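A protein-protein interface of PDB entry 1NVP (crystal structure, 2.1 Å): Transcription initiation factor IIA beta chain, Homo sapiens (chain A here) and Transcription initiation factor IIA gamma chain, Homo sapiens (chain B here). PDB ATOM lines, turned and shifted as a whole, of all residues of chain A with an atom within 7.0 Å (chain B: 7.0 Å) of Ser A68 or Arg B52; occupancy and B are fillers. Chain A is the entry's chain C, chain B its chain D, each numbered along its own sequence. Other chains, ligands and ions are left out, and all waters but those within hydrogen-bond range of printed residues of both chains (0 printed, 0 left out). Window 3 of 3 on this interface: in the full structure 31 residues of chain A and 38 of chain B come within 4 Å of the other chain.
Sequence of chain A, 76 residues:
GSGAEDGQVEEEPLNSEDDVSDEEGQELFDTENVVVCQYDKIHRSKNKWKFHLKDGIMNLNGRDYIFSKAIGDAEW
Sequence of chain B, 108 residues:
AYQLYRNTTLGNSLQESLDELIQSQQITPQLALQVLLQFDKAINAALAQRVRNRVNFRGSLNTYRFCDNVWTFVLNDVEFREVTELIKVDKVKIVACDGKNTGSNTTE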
ATOM      1  N   GLN A  38      31.650 -18.868  11.292  1.00  0.00           N
ATOM      2  CA  GLN A  38      31.032 -18.877  12.601  1.00  0.00           C
ATOM      3  C   GLN A  38      31.277 -20.278  13.136  1.00  0.00           C
ATOM      4  O   GLN A  38      31.382 -21.231  12.361  1.00  0.00           O
ATOM      5  CB  GLN A  38      29.534 -18.601  12.471  1.00  0.00           C
ATOM      6  CG  GLN A  38      29.218 -17.230  11.881  1.00  0.00           C
ATOM      7  CD  GLN A  38      27.777 -17.114  11.417  1.00  0.00           C
ATOM      8  OE1 GLN A  38      26.850 -17.431  12.159  1.00  0.00           O
ATOM      9  NE2 GLN A  38      27.584 -16.655  10.181  1.00  0.00           N
ATOM     10  N   ASP A  40      30.299 -23.614  15.692  1.00  0.00           N
ATOM     11  CA  ASP A  40      29.230 -24.308  16.391  1.00  0.00           C
ATOM     12  C   ASP A  40      29.830 -24.782  17.707  1.00  0.00           C
ATOM     13  O   ASP A  40      29.335 -24.456  18.782  1.00  0.00           O
ATOM     14  CB  ASP A  40      28.723 -25.502  15.577  1.00  0.00           C
ATOM     15  CG  ASP A  40      27.703 -25.098  14.527  1.00  0.00           C
ATOM     16  OD1 ASP A  40      26.779 -24.325  14.864  1.00  0.00           O
ATOM     17  OD2 ASP A  40      27.816 -25.560  13.371  1.00  0.00           O
ATOM     18  N   LEU A  53      32.854 -25.911  12.390  1.00  0.00           N
ATOM     19  CA  LEU A  53      32.525 -24.623  11.783  1.00  0.00           C
ATOM     20  C   LEU A  53      31.396 -24.649  10.744  1.00  0.00           C
ATOM     21  O   LEU A  53      31.027 -25.710  10.229  1.00  0.00           O
ATOM     22  CB  LEU A  53      33.794 -24.046  11.152  1.00  0.00           C
ATOM     23  CG  LEU A  53      35.036 -24.137  12.046  1.00  0.00           C
ATOM     24  CD1 LEU A  53      36.272 -23.698  11.283  1.00  0.00           C
ATOM     25  CD2 LEU A  53      34.833 -23.269  13.272  1.00  0.00           C
ATOM     26  N   LYS A  54      30.859 -23.469  10.441  1.00  0.00           N
ATOM     27  CA  LYS A  54      29.771 -23.336   9.469  1.00  0.00           C
ATOM     28  C   LYS A  54      29.770 -21.971   8.767  1.00  0.00           C
ATOM     29  O   LYS A  54      30.459 -21.037   9.189  1.00  0.00           O
ATOM     30  CB  LYS A  54      28.423 -23.535  10.161  1.00  0.00           C
ATOM     31  CG  LYS A  54      28.032 -22.382  11.074  1.00  0.00           C
ATOM     32  CD  LYS A  54      26.716 -22.655  11.774  1.00  0.00           C
ATOM     33  CE  LYS A  54      26.310 -21.489  12.655  1.00  0.00           C
ATOM     34  NZ  LYS A  54      25.094 -21.819  13.448  1.00  0.00           N
ATOM     35  N   ASP A  55      28.978 -21.867   7.702  1.00  0.00           N
ATOM     36  CA  ASP A  55      28.852 -20.633   6.923  1.00  0.00           C
ATOM     37  C   ASP A  55      30.182 -19.923   6.752  1.00  0.00           C
ATOM     38  O   ASP A  55      30.373 -18.821   7.271  1.00  0.00           O
ATOM     39  CB  ASP A  55      27.866 -19.672   7.592  1.00  0.00           C
ATOM     40  CG  ASP A  55      26.473 -20.246   7.691  1.00  0.00           C
ATOM     41  OD1 ASP A  55      26.166 -21.186   6.931  1.00  0.00           O
ATOM     42  OD2 ASP A  55      25.678 -19.748   8.518  1.00  0.00           O
ATOM     43  N   GLY A  56      31.095 -20.544   6.014  1.00  0.00           N
ATOM     44  CA  GLY A  56      32.393 -19.932   5.822  1.00  0.00           C
ATOM     45  C   GLY A  56      32.804 -19.621   4.396  1.00  0.00           C
ATOM     46  O   GLY A  56      32.455 -20.331   3.452  1.00  0.00           O
ATOM     47  N   ILE A  66      33.530 -21.796  -0.448  1.00  0.00           N
ATOM     48  CA  ILE A  66      32.466 -21.617   0.537  1.00  0.00           C
ATOM     49  C   ILE A  66      32.014 -22.958   1.112  1.00  0.00           C
ATOM     50  O   ILE A  66      32.081 -23.987   0.441  1.00  0.00           O
ATOM     51  CB  ILE A  66      31.213 -20.936  -0.074  1.00  0.00           C
ATOM     52  CG1 ILE A  66      31.561 -19.545  -0.606  1.00  0.00           C
ATOM     53  CG2 ILE A  66      30.120 -20.821   0.985  1.00  0.00           C
ATOM     54  CD1 ILE A  66      30.365 -18.792  -1.180  1.00  0.00           C
ATOM     55  N   PHE A  67      31.550 -22.939   2.357  1.00  0.00           N
ATOM     56  CA  PHE A  67      31.059 -24.152   3.001  1.00  0.00           C
ATOM     57  C   PHE A  67      29.937 -23.827   3.972  1.00  0.00           C
ATOM     58  O   PHE A  67      29.882 -22.730   4.531  1.00  0.00           O
ATOM     59  CB  PHE A  67      32.194 -24.891   3.740  1.00  0.00           C
ATOM     60  CG  PHE A  67      32.753 -24.149   4.935  1.00  0.00           C
ATOM     61  CD1 PHE A  67      31.987 -23.958   6.084  1.00  0.00           C
ATOM     62  CD2 PHE A  67      34.055 -23.657   4.911  1.00  0.00           C
ATOM     63  CE1 PHE A  67      32.506 -23.288   7.187  1.00  0.00           C
ATOM     64  CE2 PHE A  67      34.587 -22.986   6.010  1.00  0.00           C
ATOM     65  CZ  PHE A  67      33.810 -22.801   7.150  1.00  0.00           C
ATOM     66  N   SER A  68      29.032 -24.780   4.152  1.00  0.00           N
ATOM     67  CA  SER A  68      27.927 -24.611   5.082  1.00  0.00           C
ATOM     68  C   SER A  68      28.427 -25.190   6.402  1.00  0.00           C
ATOM     69  O   SER A  68      28.022 -24.768   7.485  1.00  0.00           O
ATOM     70  CB  SER A  68      26.700 -25.384   4.594  1.00  0.00           C
ATOM     71  OG  SER A  68      27.000 -26.760   4.430  1.00  0.00           O
ATOM     72  N   LYS A  69      29.330 -26.159   6.282  1.00  0.00           N
ATOM     73  CA  LYS A  69      29.925 -26.827   7.428  1.00  0.00           C
ATOM     74  C   LYS A  69      31.364 -27.238   7.150  1.00  0.00           C
ATOM     75  O   LYS A  69      31.694 -27.699   6.056  1.00  0.00           O
ATOM     76  CB  LYS A  69      29.130 -28.075   7.801  1.00  0.00           C
ATOM     77  CG  LYS A  69      27.956 -27.843   8.735  1.00  0.00           C
ATOM     78  CD  LYS A  69      27.462 -29.182   9.264  1.00  0.00           C
ATOM     79  CE  LYS A  69      28.585 -29.921   9.991  1.00  0.00           C
ATOM     80  NZ  LYS A  69      28.430 -31.403   9.937  1.00  0.00           N
ATOM     81  N   ALA A  70      32.212 -27.071   8.156  1.00  0.00           N
ATOM     82  CA  ALA A  70      33.614 -27.441   8.049  1.00  0.00           C
ATOM     83  C   ALA A  70      34.038 -28.104   9.356  1.00  0.00           C
ATOM     84  O   ALA A  70      33.782 -27.579  10.441  1.00  0.00           O
ATOM     85  CB  ALA A  70      34.469 -26.207   7.778  1.00  0.00           C
ATOM     86  N   LEU B  47      24.534 -17.166   2.506  1.00  0.00           N
ATOM     87  CA  LEU B  47      25.314 -18.301   2.988  1.00  0.00           C
ATOM     88  C   LEU B  47      24.458 -19.387   3.624  1.00  0.00           C
ATOM     89  O   LEU B  47      24.551 -20.560   3.261  1.00  0.00           O
ATOM     90  CB  LEU B  47      26.359 -17.831   4.001  1.00  0.00           C
ATOM     91  CG  LEU B  47      27.577 -17.115   3.425  1.00  0.00           C
ATOM     92  CD1 LEU B  47      28.456 -16.625   4.551  1.00  0.00           C
ATOM     93  CD2 LEU B  47      28.345 -18.064   2.520  1.00  0.00           C
ATOM     94  N   ALA B  48      23.623 -18.984   4.573  1.00  0.00           N
ATOM     95  CA  ALA B  48      22.759 -19.916   5.284  1.00  0.00           C
ATOM     96  C   ALA B  48      21.723 -20.602   4.399  1.00  0.00           C
ATOM     97  O   ALA B  48      21.508 -21.810   4.509  1.00  0.00           O
ATOM     98  CB  ALA B  48      22.064 -19.194   6.429  1.00  0.00           C
ATOM     99  N   GLN B  49      21.088 -19.836   3.519  1.00  0.00           N
ATOM    100  CA  GLN B  49      20.055 -20.385   2.646  1.00  0.00           C
ATOM    101  C   GLN B  49      20.548 -20.986   1.333  1.00  0.00           C
ATOM    102  O   GLN B  49      19.979 -21.963   0.846  1.00  0.00           O
ATOM    103  CB  GLN B  49      19.009 -19.314   2.360  1.00  0.00           C
ATOM    104  N   ARG B  50      21.605 -20.418   0.761  1.00  0.00           N
ATOM    105  CA  ARG B  50      22.116 -20.902  -0.520  1.00  0.00           C
ATOM    106  C   ARG B  50      23.110 -22.064  -0.479  1.00  0.00           C
ATOM    107  O   ARG B  50      22.779 -23.175  -0.893  1.00  0.00           O
ATOM    108  CB  ARG B  50      22.710 -19.740  -1.310  1.00  0.00           C
ATOM    109  N   VAL B  51      24.325 -21.810  -0.001  1.00  0.00           N
ATOM    110  CA  VAL B  51      25.345 -22.859   0.058  1.00  0.00           C
ATOM    111  C   VAL B  51      24.915 -23.986   0.998  1.00  0.00           C
ATOM    112  O   VAL B  51      24.198 -23.745   1.970  1.00  0.00           O
ATOM    113  CB  VAL B  51      26.700 -22.288   0.525  1.00  0.00           C
ATOM    114  CG1 VAL B  51      27.799 -23.323   0.325  1.00  0.00           C
ATOM    115  CG2 VAL B  51      27.016 -21.015  -0.246  1.00  0.00           C
ATOM    116  N   ARG B  52      25.352 -25.212   0.716  1.00  0.00           N
ATOM    117  CA  ARG B  52      24.968 -26.351   1.550  1.00  0.00           C
ATOM    118  C   ARG B  52      25.909 -27.560   1.502  1.00  0.00           C
ATOM    119  O   ARG B  52      25.470 -28.695   1.693  1.00  0.00           O
ATOM    120  CB  ARG B  52      23.553 -26.790   1.180  1.00  0.00           C
ATOM    121  N   ASN B  53      27.195 -27.326   1.265  1.00  0.00           N
ATOM    122  CA  ASN B  53      28.164 -28.420   1.192  1.00  0.00           C
ATOM    123  C   ASN B  53      29.050 -28.515   2.435  1.00  0.00           C
ATOM    124  O   ASN B  53      29.127 -27.577   3.231  1.00  0.00           O
ATOM    125  CB  ASN B  53      29.032 -28.253  -0.052  1.00  0.00           C
ATOM    126  CG  ASN B  53      29.722 -26.912  -0.096  1.00  0.00           C
ATOM    127  OD1 ASN B  53      29.106 -25.878   0.155  1.00  0.00           O
ATOM    128  ND2 ASN B  53      31.006 -26.917  -0.420  1.00  0.00           N
ATOM    129  N   ARG B  54      29.724 -29.652   2.586  1.00  0.00           N
ATOM    130  CA  ARG B  54      30.595 -29.888   3.734  1.00  0.00           C
ATOM    131  C   ARG B  54      32.075 -29.952   3.365  1.00  0.00           C
ATOM    132  O   ARG B  54      32.442 -30.431   2.294  1.00  0.00           O
ATOM    133  CB  ARG B  54      30.173 -31.182   4.439  1.00  0.00           C
ATOM    134  CG  ARG B  54      31.075 -31.621   5.585  1.00  0.00           C
ATOM    135  CD  ARG B  54      30.419 -32.753   6.364  1.00  0.00           C
ATOM    136  NE  ARG B  54      31.370 -33.505   7.178  1.00  0.00           N
ATOM    137  CZ  ARG B  54      31.046 -34.563   7.914  1.00  0.00           C
ATOM    138  NH1 ARG B  54      29.792 -34.996   7.943  1.00  0.00           N
ATOM    139  NH2 ARG B  54      31.978 -35.199   8.613  1.00  0.00           N
ATOM    140  N   VAL B  55      32.913 -29.462   4.273  1.00  0.00           N
ATOM    141  CA  VAL B  55      34.360 -29.444   4.084  1.00  0.00           C
ATOM    142  C   VAL B  55      35.054 -30.057   5.303  1.00  0.00           C
ATOM    143  O   VAL B  55      34.471 -30.140   6.385  1.00  0.00           O
ATOM    144  CB  VAL B  55      34.872 -27.992   3.894  1.00  0.00           C
ATOM    145  CG1 VAL B  55      36.393 -27.968   3.820  1.00  0.00           C
ATOM    146  CG2 VAL B  55      34.276 -27.395   2.629  1.00  0.00           C
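The backbone carbonyl oxygen (O) of Lys A69 lies within hydrogen-bond range of the backbone NH (N) of Val B55, 2.8 Å away. The backbone carbonyl oxygen (O) of Ile A66 lies within hydrogen-bond range of the side-chain amide nitrogen (ND2) of Asn B53 (3.2 Å). O of Asn B53 sits at hydrogen-bond distance from N of Lys A69 (3.4 Å). The side-chain hydroxyl (OG) of Ser A68 lies within hydrogen-bond range of the backbone carbonyl oxygen (O) of Asn B53 (2.6 Å).
The backbone NH (N) of Asp A55 lies close to the backbone carbonyl oxygen (O) of Phe A67. N of Gly A56 lies within hydrogen-bond range of O of Phe A67. The backbone NH (N) of Asp A55 is in hydrogen-bond range of the backbone carbonyl oxygen (O) of Ser A68, at 3.1 Å. N of Leu A53 lies within hydrogen-bond range of O of Ala A70, at 2.7 Å.
Printed residues of chain B within 4 Å of Ser A68: Val B51, Arg B52 and Asn B53. Of chain A, only Ser A68 comes within 4 Å of Arg B52. Of the printed residues of chain A, Leu B47 touches Asp A55 (3.99 Å) and Ile A66 (3.6 Å). Of the printed residues of chain A, Val B51 touches Ile A66 (3.3 Å) and Ser A68 (3.98 Å). Of the printed residues of chain B, Lys A69 touches Asn B53, Arg B54 and Val B55. Printed residues of chain B within 4 Å of Ala A70: Val B55 (3.3 Å). Of the printed residues of chain A, Arg B54 touches Lys A69 (3.4 Å).
Asp A55 touches Leu B47 (O to CD1, 3.99 Å). OD1 of Asp A55 touches CA of Ala B48, 3.99 Å away. Ile A66 touches Leu B47. CG2 of Ile A66 touches CG2 of Val B51, 3.3 Å away. Phe A67 touches Asn B53 (CA to OD1, 3.9 Å). Val B55 touches Phe A67 (CG2 to CB, 3.4 Å). Val B51 touches Ser A68 (O to CB, 3.98 Å). Ser A68 touches Arg B52. Lys A69 touches Arg B54. Ala A70 touches Val B55 (CA to O, 3.3 Å).
Printed residues of chain B that touch a printed residue of chain A: Leu B47, Ala B48, Val B51, Arg B52, Asn B53, Arg B54 and Val B55. Of the 11 printed residues of chain A, 6 touch a printed residue of chain B. Hydrophobic or aromatic side chains of chain A that line the printed part of chain B: Ile A66 and Phe A67. Among the printed residues, 14 pairs touch across the chains. Among the printed residues, no Asp or Glu carboxylate lies within 4 Å of a Lys or Arg side-chain nitrogen of the other chain.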
